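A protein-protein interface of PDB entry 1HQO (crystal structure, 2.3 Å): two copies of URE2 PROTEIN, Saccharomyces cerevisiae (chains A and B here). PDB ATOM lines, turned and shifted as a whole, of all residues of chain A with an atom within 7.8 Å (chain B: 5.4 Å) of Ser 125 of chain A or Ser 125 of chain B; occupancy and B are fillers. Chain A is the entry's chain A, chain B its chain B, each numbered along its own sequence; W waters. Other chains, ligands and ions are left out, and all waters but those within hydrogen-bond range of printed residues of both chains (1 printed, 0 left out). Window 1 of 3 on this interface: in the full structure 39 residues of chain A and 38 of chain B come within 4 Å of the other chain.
The side-chain hydroxyl (OG1) of Thr 124 of chain A is in hydrogen-bond range of the side-chain hydroxyl (OG) of Ser 125 of chain A, at 3.3 Å. O of Leu 120 of chain A is in hydrogen-bond range of OG1 of Thr 124 of chain A, 3.1 Å away. NE2 of Gln 133 of chain A sits close to O of Pro 129 of chain A, at 3.4 Å. The side-chain hydroxyl (OG) of Ser 125 of chain A lies close to the backbone carbonyl oxygen (O) of Phe 121 of chain A. O of Phe 121 of chain B is in hydrogen-bond range of OG1 of Thr 124 of chain B (3.3 Å). O of Phe 121 of chain B sits at hydrogen-bond distance from OG of Ser 125 of chain B (2.4 Å).
The backbone NH (N) of Ser 125 of chain B lies close to the side-chain hydroxyl (OG) of Ser 125 of chain A. The side-chain hydroxyl (OG1) of Thr 124 of chain B is in hydrogen-bond range of the side-chain hydroxyl (OG) of Ser 125 of chain A (3.2 Å).
Of the printed residues of chain B, Gly 86 of chain A touches Phe 121 (3.6 Å). Of the printed residues of chain B, Phe 122 of chain A touches Glu 84 (3.2 Å). Printed residues of chain B within 4 Å of Thr 124 of chain A: Phe 121 and Ser 125. Ser 125 of chain A touches three residues of chain B. His 127 of chain A touches none of the printed residues of chain B. Printed residues of chain A within 4 Å of Phe 121 of chain B: Gly 86 (3.6 Å), Leu 120 (3.7 Å), Phe 121 (3.4 Å) and Thr 124 (3.4 Å). Ser 125 of chain B touches just these residues of chain A: Thr 124, Ser 125 and Pro 129. The nearest residue of chain B that does not touch Ser 125 of chain A is Phe 121 of chain B (4.7 Å). The nearest residue of chain A that does not touch Ser 125 of chain B is Glu 84 of chain A (4.1 Å).
Of the 11 printed residues of chain B, 7 touch a printed residue of chain A. Hydrophobic or aromatic side chains of chain B within 4 Å of the printed part of chain A: Leu 120, Phe 121, Phe 122 and Pro 129. Hydrophobic or aromatic side chains of chain A that line the printed part of chain B: Leu 120, Phe 121, Phe 122 and Pro 129. Among the printed residues, 15 pairs touch across the chains.
Glu 84 of chain A touches Phe 122 of chain B. CE1 of Phe 121 of chain B touches C of Gly 86 of chain A, 3.6 Å away. Ala 118 of chain A touches Glu 84 of chain B (O to CG, 3.3 Å). Leu 120 of chain A touches Phe 121 of chain B (CD2 to CZ, 3.7 Å). Glu 84 of chain B touches Phe 121 of chain A. Phe 121 of chain A touches Leu 120 of chain B. Phe 121 of chain B touches Phe 121 of chain A. Glu 84 of chain B touches Phe 122 of chain A. Thr 124 of chain A touches Phe 121 of chain B (OG1 to CE2, 3.4 Å). Thr 124 of chain A touches Ser 125 of chain B (O to CB, 3.3 Å).
Water W1 bridges OE1 of Glu 84 of chain A and OG of Ser 125 of chain B.
Leu 120 of chain A touches Phe 121 of chain B, and with the chains exchanged Phe 121 of chain A touches Leu 120 of chain B. Phe 121 of chain B touches its own counterpart, Phe 121 of chain A. Ser 125 of chain A touches its own counterpart, Ser 125 of chain B. Ser 125 of chain A touches Pro 129 of chain B, and with the chains exchanged Pro 129 of chain A touches Ser 125 of chain B. 11 positions are printed for both chains. Of the 15 pairs that touch across the chains among the printed residues, 12 have their exchanged pair printed and touching as well.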
ATOM      1  N   ASN A  28      17.300  -9.782   8.001  1.00  0.00           N
ATOM      2  CA  ASN A  28      18.052  -8.608   8.424  1.00  0.00           C
ATOM      3  C   ASN A  28      17.459  -8.037   9.673  1.00  0.00           C
ATOM      4  O   ASN A  28      18.096  -7.276  10.393  1.00  0.00           O
ATOM      5  CB  ASN A  28      18.080  -7.566   7.325  1.00  0.00           C
ATOM      6  CG  ASN A  28      19.137  -7.866   6.310  1.00  0.00           C
ATOM      7  OD1 ASN A  28      20.161  -8.473   6.636  1.00  0.00           O
ATOM      8  ND2 ASN A  28      18.915  -7.439   5.073  1.00  0.00           N
ATOM      9  N   LYS A  31      18.616 -10.057  12.532  1.00  0.00           N
ATOM     10  CA  LYS A  31      20.027  -9.748  12.599  1.00  0.00           C
ATOM     11  C   LYS A  31      20.257  -8.623  13.603  1.00  0.00           C
ATOM     12  O   LYS A  31      21.185  -8.663  14.377  1.00  0.00           O
ATOM     13  CB  LYS A  31      20.538  -9.315  11.229  1.00  0.00           C
ATOM     14  CG  LYS A  31      22.035  -9.055  11.207  1.00  0.00           C
ATOM     15  CD  LYS A  31      22.547  -8.661   9.837  1.00  0.00           C
ATOM     16  CE  LYS A  31      22.250  -7.221   9.539  1.00  0.00           C
ATOM     17  NZ  LYS A  31      22.772  -6.867   8.200  1.00  0.00           N
ATOM     18  N   GLU A  84      18.991   1.090   8.165  1.00  0.00           N
ATOM     19  CA  GLU A  84      19.615   0.042   7.351  1.00  0.00           C
ATOM     20  C   GLU A  84      20.278  -0.886   8.365  1.00  0.00           C
ATOM     21  O   GLU A  84      20.988  -0.402   9.242  1.00  0.00           O
ATOM     22  CB  GLU A  84      20.670   0.622   6.414  1.00  0.00           C
ATOM     23  CG  GLU A  84      20.152   1.089   5.055  1.00  0.00           C
ATOM     24  CD  GLU A  84      19.813  -0.051   4.074  1.00  0.00           C
ATOM     25  OE1 GLU A  84      20.019  -1.252   4.392  1.00  0.00           O
ATOM     26  OE2 GLU A  84      19.335   0.264   2.958  1.00  0.00           O
ATOM     27  N   SER A  85      20.057  -2.202   8.257  1.00  0.00           N
ATOM     28  CA  SER A  85      20.631  -3.166   9.218  1.00  0.00           C
ATOM     29  C   SER A  85      22.128  -3.019   9.489  1.00  0.00           C
ATOM     30  O   SER A  85      22.562  -3.172  10.632  1.00  0.00           O
ATOM     31  CB  SER A  85      20.342  -4.602   8.790  1.00  0.00           C
ATOM     32  OG  SER A  85      20.960  -4.901   7.555  1.00  0.00           O
ATOM     33  N   GLY A  86      22.909  -2.742   8.442  1.00  0.00           N
ATOM     34  CA  GLY A  86      24.335  -2.541   8.595  1.00  0.00           C
ATOM     35  C   GLY A  86      24.659  -1.278   9.386  1.00  0.00           C
ATOM     36  O   GLY A  86      25.589  -1.277  10.179  1.00  0.00           O
ATOM     37  N   ALA A 118      34.348  -4.617   6.206  1.00  0.00           N
ATOM     38  CA  ALA A 118      34.453  -5.313   4.932  1.00  0.00           C
ATOM     39  C   ALA A 118      33.507  -6.502   4.889  1.00  0.00           C
ATOM     40  O   ALA A 118      32.810  -6.683   3.909  1.00  0.00           O
ATOM     41  CB  ALA A 118      35.880  -5.787   4.701  1.00  0.00           C
ATOM     42  N   TRP A 119      33.495  -7.315   5.947  1.00  0.00           N
ATOM     43  CA  TRP A 119      32.629  -8.486   6.007  1.00  0.00           C
ATOM     44  C   TRP A 119      31.176  -8.076   6.141  1.00  0.00           C
ATOM     45  O   TRP A 119      30.295  -8.755   5.619  1.00  0.00           O
ATOM     46  CB  TRP A 119      33.006  -9.431   7.175  1.00  0.00           C
ATOM     47  CG  TRP A 119      34.273 -10.223   6.928  1.00  0.00           C
ATOM     48  CD1 TRP A 119      35.507  -9.965   7.441  1.00  0.00           C
ATOM     49  CD2 TRP A 119      34.456 -11.278   5.974  1.00  0.00           C
ATOM     50  NE1 TRP A 119      36.451 -10.771   6.854  1.00  0.00           N
ATOM     51  CE2 TRP A 119      35.835 -11.585   5.947  1.00  0.00           C
ATOM     52  CE3 TRP A 119      33.590 -11.980   5.125  1.00  0.00           C
ATOM     53  CZ2 TRP A 119      36.370 -12.564   5.115  1.00  0.00           C
ATOM     54  CZ3 TRP A 119      34.117 -12.951   4.300  1.00  0.00           C
ATOM     55  CH2 TRP A 119      35.503 -13.233   4.297  1.00  0.00           C
ATOM     56  N   LEU A 120      30.922  -6.964   6.829  1.00  0.00           N
ATOM     57  CA  LEU A 120      29.550  -6.491   7.018  1.00  0.00           C
ATOM     58  C   LEU A 120      28.948  -6.012   5.686  1.00  0.00           C
ATOM     59  O   LEU A 120      27.821  -6.354   5.333  1.00  0.00           O
ATOM     60  CB  LEU A 120      29.515  -5.363   8.062  1.00  0.00           C
ATOM     61  CG  LEU A 120      28.139  -4.765   8.399  1.00  0.00           C
ATOM     62  CD1 LEU A 120      27.189  -5.844   8.876  1.00  0.00           C
ATOM     63  CD2 LEU A 120      28.289  -3.707   9.451  1.00  0.00           C
ATOM     64  N   PHE A 121      29.706  -5.211   4.949  1.00  0.00           N
ATOM     65  CA  PHE A 121      29.251  -4.732   3.666  1.00  0.00           C
ATOM     66  C   PHE A 121      29.166  -5.902   2.703  1.00  0.00           C
ATOM     67  O   PHE A 121      28.322  -5.923   1.814  1.00  0.00           O
ATOM     68  CB  PHE A 121      30.201  -3.662   3.107  1.00  0.00           C
ATOM     69  CG  PHE A 121      29.915  -2.262   3.609  1.00  0.00           C
ATOM     70  CD1 PHE A 121      30.490  -1.788   4.780  1.00  0.00           C
ATOM     71  CD2 PHE A 121      29.061  -1.421   2.901  1.00  0.00           C
ATOM     72  CE1 PHE A 121      30.217  -0.494   5.231  1.00  0.00           C
ATOM     73  CE2 PHE A 121      28.790  -0.140   3.344  1.00  0.00           C
ATOM     74  CZ  PHE A 121      29.367   0.327   4.508  1.00  0.00           C
ATOM     75  N   PHE A 122      30.039  -6.882   2.874  1.00  0.00           N
ATOM     76  CA  PHE A 122      30.019  -8.045   2.006  1.00  0.00           C
ATOM     77  C   PHE A 122      28.687  -8.798   2.199  1.00  0.00           C
ATOM     78  O   PHE A 122      28.005  -9.182   1.238  1.00  0.00           O
ATOM     79  CB  PHE A 122      31.216  -8.945   2.328  1.00  0.00           C
ATOM     80  CG  PHE A 122      31.322 -10.160   1.447  1.00  0.00           C
ATOM     81  CD1 PHE A 122      31.144 -10.062   0.069  1.00  0.00           C
ATOM     82  CD2 PHE A 122      31.587 -11.405   1.995  1.00  0.00           C
ATOM     83  CE1 PHE A 122      31.220 -11.180  -0.747  1.00  0.00           C
ATOM     84  CE2 PHE A 122      31.667 -12.542   1.181  1.00  0.00           C
ATOM     85  CZ  PHE A 122      31.482 -12.425  -0.187  1.00  0.00           C
ATOM     86  N   GLN A 123      28.308  -8.993   3.450  1.00  0.00           N
ATOM     87  CA  GLN A 123      27.065  -9.676   3.734  1.00  0.00           C
ATOM     88  C   GLN A 123      25.871  -8.862   3.261  1.00  0.00           C
ATOM     89  O   GLN A 123      25.043  -9.355   2.493  1.00  0.00           O
ATOM     90  CB  GLN A 123      26.937  -9.944   5.231  1.00  0.00           C
ATOM     91  CG  GLN A 123      25.682 -10.713   5.618  1.00  0.00           C
ATOM     92  CD  GLN A 123      24.501  -9.809   5.915  1.00  0.00           C
ATOM     93  OE1 GLN A 123      24.621  -8.817   6.618  1.00  0.00           O
ATOM     94  NE2 GLN A 123      23.351 -10.162   5.396  1.00  0.00           N
ATOM     95  N   THR A 124      25.787  -7.607   3.694  1.00  0.00           N
ATOM     96  CA  THR A 124      24.660  -6.777   3.319  1.00  0.00           C
ATOM     97  C   THR A 124      24.504  -6.497   1.825  1.00  0.00           C
ATOM     98  O   THR A 124      23.391  -6.497   1.305  1.00  0.00           O
ATOM     99  CB  THR A 124      24.686  -5.429   4.038  1.00  0.00           C
ATOM    100  OG1 THR A 124      25.844  -4.689   3.636  1.00  0.00           O
ATOM    101  CG2 THR A 124      24.683  -5.627   5.532  1.00  0.00           C
ATOM    102  N   SER A 125      25.606  -6.295   1.120  1.00  0.00           N
ATOM    103  CA  SER A 125      25.501  -5.963  -0.277  1.00  0.00           C
ATOM    104  C   SER A 125      25.897  -7.019  -1.251  1.00  0.00           C
ATOM    105  O   SER A 125      25.644  -6.859  -2.439  1.00  0.00           O
ATOM    106  CB  SER A 125      26.311  -4.717  -0.530  1.00  0.00           C
ATOM    107  OG  SER A 125      25.996  -3.778   0.498  1.00  0.00           O
ATOM    108  N   GLY A 126      26.521  -8.098  -0.792  1.00  0.00           N
ATOM    109  CA  GLY A 126      26.908  -9.110  -1.754  1.00  0.00           C
ATOM    110  C   GLY A 126      26.231 -10.445  -1.532  1.00  0.00           C
ATOM    111  O   GLY A 126      26.063 -11.263  -2.441  1.00  0.00           O
ATOM    112  N   HIS A 127      25.790 -10.640  -0.305  1.00  0.00           N
ATOM    113  CA  HIS A 127      25.195 -11.893   0.109  1.00  0.00           C
ATOM    114  C   HIS A 127      23.646 -11.804   0.219  1.00  0.00           C
ATOM    115  O   HIS A 127      22.920 -12.432  -0.559  1.00  0.00           O
ATOM    116  CB  HIS A 127      25.934 -12.245   1.419  1.00  0.00           C
ATOM    117  CG  HIS A 127      25.579 -13.560   2.034  1.00  0.00           C
ATOM    118  ND1 HIS A 127      24.646 -13.677   3.056  1.00  0.00           N
ATOM    119  CD2 HIS A 127      26.101 -14.801   1.860  1.00  0.00           C
ATOM    120  CE1 HIS A 127      24.609 -14.927   3.486  1.00  0.00           C
ATOM    121  NE2 HIS A 127      25.483 -15.631   2.776  1.00  0.00           N
ATOM    122  N   ALA A 128      23.128 -11.001   1.138  1.00  0.00           N
ATOM    123  CA  ALA A 128      21.679 -10.911   1.296  1.00  0.00           C
ATOM    124  C   ALA A 128      20.962 -10.618  -0.007  1.00  0.00           C
ATOM    125  O   ALA A 128      20.047 -11.333  -0.376  1.00  0.00           O
ATOM    126  CB  ALA A 128      21.323  -9.852   2.334  1.00  0.00           C
ATOM    127  N   PRO A 129      21.368  -9.558  -0.723  1.00  0.00           N
ATOM    128  CA  PRO A 129      20.725  -9.205  -1.984  1.00  0.00           C
ATOM    129  C   PRO A 129      20.630 -10.365  -2.950  1.00  0.00           C
ATOM    130  O   PRO A 129      19.611 -10.552  -3.609  1.00  0.00           O
ATOM    131  CB  PRO A 129      21.620  -8.103  -2.527  1.00  0.00           C
ATOM    132  CG  PRO A 129      22.098  -7.454  -1.324  1.00  0.00           C
ATOM    133  CD  PRO A 129      22.458  -8.614  -0.439  1.00  0.00           C
ATOM    134  N   MET A 130      21.694 -11.148  -3.035  1.00  0.00           N
ATOM    135  CA  MET A 130      21.714 -12.256  -3.964  1.00  0.00           C
ATOM    136  C   MET A 130      20.771 -13.344  -3.563  1.00  0.00           C
ATOM    137  O   MET A 130      20.131 -13.943  -4.414  1.00  0.00           O
ATOM    138  CB  MET A 130      23.125 -12.807  -4.103  1.00  0.00           C
ATOM    139  CG  MET A 130      24.090 -11.796  -4.689  1.00  0.00           C
ATOM    140  SD  MET A 130      23.581 -11.030  -6.454  1.00  0.00           S
ATOM    141  CE  MET A 130      23.018  -9.255  -5.917  1.00  0.00           C
ATOM    142  N   GLN A 133      17.249 -12.285  -4.427  1.00  0.00           N
ATOM    143  CA  GLN A 133      16.909 -12.425  -5.839  1.00  0.00           C
ATOM    144  C   GLN A 133      16.676 -13.860  -6.245  1.00  0.00           C
ATOM    145  O   GLN A 133      15.877 -14.132  -7.130  1.00  0.00           O
ATOM    146  CB  GLN A 133      18.007 -11.838  -6.727  1.00  0.00           C
ATOM    147  CG  GLN A 133      18.343 -10.393  -6.434  1.00  0.00           C
ATOM    148  CD  GLN A 133      17.107  -9.555  -6.234  1.00  0.00           C
ATOM    149  OE1 GLN A 133      16.283  -9.413  -7.142  1.00  0.00           O
ATOM    150  NE2 GLN A 133      16.961  -8.992  -5.031  1.00  0.00           N
ATOM    151  N   GLU A 155      25.551 -17.341  -7.615  1.00  0.00           N
ATOM    152  CA  GLU A 155      26.243 -16.271  -6.931  1.00  0.00           C
ATOM    153  C   GLU A 155      26.199 -16.462  -5.419  1.00  0.00           C
ATOM    154  O   GLU A 155      27.156 -16.117  -4.728  1.00  0.00           O
ATOM    155  CB  GLU A 155      25.665 -14.921  -7.311  1.00  0.00           C
ATOM    156  CG  GLU A 155      26.323 -13.766  -6.552  1.00  0.00           C
ATOM    157  CD  GLU A 155      27.803 -13.609  -6.834  1.00  0.00           C
ATOM    158  OE1 GLU A 155      28.387 -14.469  -7.513  1.00  0.00           O
ATOM    159  OE2 GLU A 155      28.384 -12.617  -6.366  1.00  0.00           O
ATOM    160  N   VAL A 159      29.558 -16.655  -3.122  1.00  0.00           N
ATOM    161  CA  VAL A 159      29.760 -15.824  -1.959  1.00  0.00           C
ATOM    162  C   VAL A 159      29.951 -16.681  -0.721  1.00  0.00           C
ATOM    163  O   VAL A 159      30.703 -16.308   0.175  1.00  0.00           O
ATOM    164  CB  VAL A 159      28.589 -14.845  -1.772  1.00  0.00           C
ATOM    165  CG1 VAL A 159      28.522 -14.333  -0.308  1.00  0.00           C
ATOM    166  CG2 VAL A 159      28.788 -13.681  -2.689  1.00  0.00           C
ATOM    167  N   GLU B  84      35.983  -3.774   0.372  1.00  0.00           N
ATOM    168  CA  GLU B  84      34.583  -3.446   0.034  1.00  0.00           C
ATOM    169  C   GLU B  84      34.528  -1.925  -0.017  1.00  0.00           C
ATOM    170  O   GLU B  84      34.944  -1.269   0.946  1.00  0.00           O
ATOM    171  CB  GLU B  84      33.586  -3.978   1.082  1.00  0.00           C
ATOM    172  CG  GLU B  84      33.131  -5.441   0.887  1.00  0.00           C
ATOM    173  CD  GLU B  84      32.075  -5.650  -0.222  1.00  0.00           C
ATOM    174  OE1 GLU B  84      31.626  -4.663  -0.855  1.00  0.00           O
ATOM    175  OE2 GLU B  84      31.684  -6.819  -0.457  1.00  0.00           O
ATOM    176  N   LEU B 120      24.924   5.157   3.081  1.00  0.00           N
ATOM    177  CA  LEU B 120      26.055   4.451   2.467  1.00  0.00           C
ATOM    178  C   LEU B 120      25.677   2.985   2.218  1.00  0.00           C
ATOM    179  O   LEU B 120      25.929   2.432   1.142  1.00  0.00           O
ATOM    180  CB  LEU B 120      27.273   4.549   3.391  1.00  0.00           C
ATOM    181  CG  LEU B 120      28.558   3.850   2.959  1.00  0.00           C
ATOM    182  CD1 LEU B 120      28.985   4.348   1.588  1.00  0.00           C
ATOM    183  CD2 LEU B 120      29.635   4.109   3.977  1.00  0.00           C
ATOM    184  N   PHE B 121      25.075   2.366   3.228  1.00  0.00           N
ATOM    185  CA  PHE B 121      24.608   0.989   3.129  1.00  0.00           C
ATOM    186  C   PHE B 121      23.419   0.866   2.172  1.00  0.00           C
ATOM    187  O   PHE B 121      23.223  -0.159   1.545  1.00  0.00           O
ATOM    188  CB  PHE B 121      24.193   0.471   4.502  1.00  0.00           C
ATOM    189  CG  PHE B 121      25.304  -0.190   5.266  1.00  0.00           C
ATOM    190  CD1 PHE B 121      26.025   0.518   6.213  1.00  0.00           C
ATOM    191  CD2 PHE B 121      25.614  -1.535   5.044  1.00  0.00           C
ATOM    192  CE1 PHE B 121      27.028  -0.095   6.930  1.00  0.00           C
ATOM    193  CE2 PHE B 121      26.618  -2.159   5.758  1.00  0.00           C
ATOM    194  CZ  PHE B 121      27.328  -1.437   6.706  1.00  0.00           C
ATOM    195  N   PHE B 122      22.618   1.915   2.083  1.00  0.00           N
ATOM    196  CA  PHE B 122      21.488   1.920   1.186  1.00  0.00           C
ATOM    197  C   PHE B 122      22.034   1.948  -0.228  1.00  0.00           C
ATOM    198  O   PHE B 122      21.565   1.246  -1.116  1.00  0.00           O
ATOM    199  CB  PHE B 122      20.645   3.159   1.449  1.00  0.00           C
ATOM    200  CG  PHE B 122      19.433   3.277   0.570  1.00  0.00           C
ATOM    201  CD1 PHE B 122      18.625   2.172   0.321  1.00  0.00           C
ATOM    202  CD2 PHE B 122      19.079   4.508   0.026  1.00  0.00           C
ATOM    203  CE1 PHE B 122      17.483   2.285  -0.450  1.00  0.00           C
ATOM    204  CE2 PHE B 122      17.934   4.640  -0.751  1.00  0.00           C
ATOM    205  CZ  PHE B 122      17.127   3.521  -0.992  1.00  0.00           C
ATOM    206  N   GLN B 123      23.042   2.778  -0.432  1.00  0.00           N
ATOM    207  CA  GLN B 123      23.644   2.892  -1.734  1.00  0.00           C
ATOM    208  C   GLN B 123      24.348   1.566  -2.108  1.00  0.00           C
ATOM    209  O   GLN B 123      24.071   0.991  -3.148  1.00  0.00           O
ATOM    210  CB  GLN B 123      24.616   4.072  -1.716  1.00  0.00           C
ATOM    211  CG  GLN B 123      25.227   4.446  -3.062  1.00  0.00           C
ATOM    212  CD  GLN B 123      26.183   3.390  -3.638  1.00  0.00           C
ATOM    213  OE1 GLN B 123      27.199   3.025  -3.021  1.00  0.00           O
ATOM    214  NE2 GLN B 123      25.861   2.903  -4.835  1.00  0.00           N
ATOM    215  N   THR B 124      25.217   1.053  -1.246  1.00  0.00           N
ATOM    216  CA  THR B 124      25.956  -0.154  -1.572  1.00  0.00           C
ATOM    217  C   THR B 124      25.153  -1.420  -1.688  1.00  0.00           C
ATOM    218  O   THR B 124      25.486  -2.301  -2.481  1.00  0.00           O
ATOM    219  CB  THR B 124      27.013  -0.464  -0.533  1.00  0.00           C
ATOM    220  OG1 THR B 124      26.365  -0.626   0.738  1.00  0.00           O
ATOM    221  CG2 THR B 124      28.057   0.643  -0.461  1.00  0.00           C
ATOM    222  N   SER B 125      24.109  -1.536  -0.877  1.00  0.00           N
ATOM    223  CA  SER B 125      23.318  -2.758  -0.872  1.00  0.00           C
ATOM    224  C   SER B 125      21.911  -2.693  -1.449  1.00  0.00           C
ATOM    225  O   SER B 125      21.281  -3.729  -1.633  1.00  0.00           O
ATOM    226  CB  SER B 125      23.251  -3.308   0.551  1.00  0.00           C
ATOM    227  OG  SER B 125      22.507  -2.456   1.386  1.00  0.00           O
ATOM    228  N   GLY B 126      21.400  -1.510  -1.741  1.00  0.00           N
ATOM    229  CA  GLY B 126      20.059  -1.475  -2.282  1.00  0.00           C
ATOM    230  C   GLY B 126      19.989  -0.795  -3.628  1.00  0.00           C
ATOM    231  O   GLY B 126      19.087  -1.042  -4.427  1.00  0.00           O
ATOM    232  N   HIS B 127      20.981   0.046  -3.871  1.00  0.00           N
ATOM    233  CA  HIS B 127      21.080   0.851  -5.075  1.00  0.00           C
ATOM    234  C   HIS B 127      22.036   0.194  -6.092  1.00  0.00           C
ATOM    235  O   HIS B 127      21.596  -0.312  -7.128  1.00  0.00           O
ATOM    236  CB  HIS B 127      21.501   2.268  -4.599  1.00  0.00           C
ATOM    237  CG  HIS B 127      21.535   3.313  -5.666  1.00  0.00           C
ATOM    238  ND1 HIS B 127      22.702   3.663  -6.326  1.00  0.00           N
ATOM    239  CD2 HIS B 127      20.559   4.101  -6.176  1.00  0.00           C
ATOM    240  CE1 HIS B 127      22.441   4.621  -7.200  1.00  0.00           C
ATOM    241  NE2 HIS B 127      21.148   4.903  -7.130  1.00  0.00           N
ATOM    242  N   ALA B 128      23.324   0.155  -5.777  1.00  0.00           N
ATOM    243  CA  ALA B 128      24.314  -0.457  -6.661  1.00  0.00           C
ATOM    244  C   ALA B 128      23.977  -1.870  -7.167  1.00  0.00           C
ATOM    245  O   ALA B 128      24.090  -2.136  -8.359  1.00  0.00           O
ATOM    246  CB  ALA B 128      25.657  -0.476  -5.975  1.00  0.00           C
ATOM    247  N   PRO B 129      23.584  -2.803  -6.267  1.00  0.00           N
ATOM    248  CA  PRO B 129      23.252  -4.165  -6.715  1.00  0.00           C
ATOM    249  C   PRO B 129      22.076  -4.213  -7.689  1.00  0.00           C
ATOM    250  O   PRO B 129      22.052  -5.045  -8.589  1.00  0.00           O
ATOM    251  CB  PRO B 129      22.913  -4.893  -5.420  1.00  0.00           C
ATOM    252  CG  PRO B 129      23.651  -4.132  -4.375  1.00  0.00           C
ATOM    253  CD  PRO B 129      23.482  -2.704  -4.797  1.00  0.00           C
HETATM  254  O   HOH W   1      19.459  -3.248   2.891  1.00  0.00           O
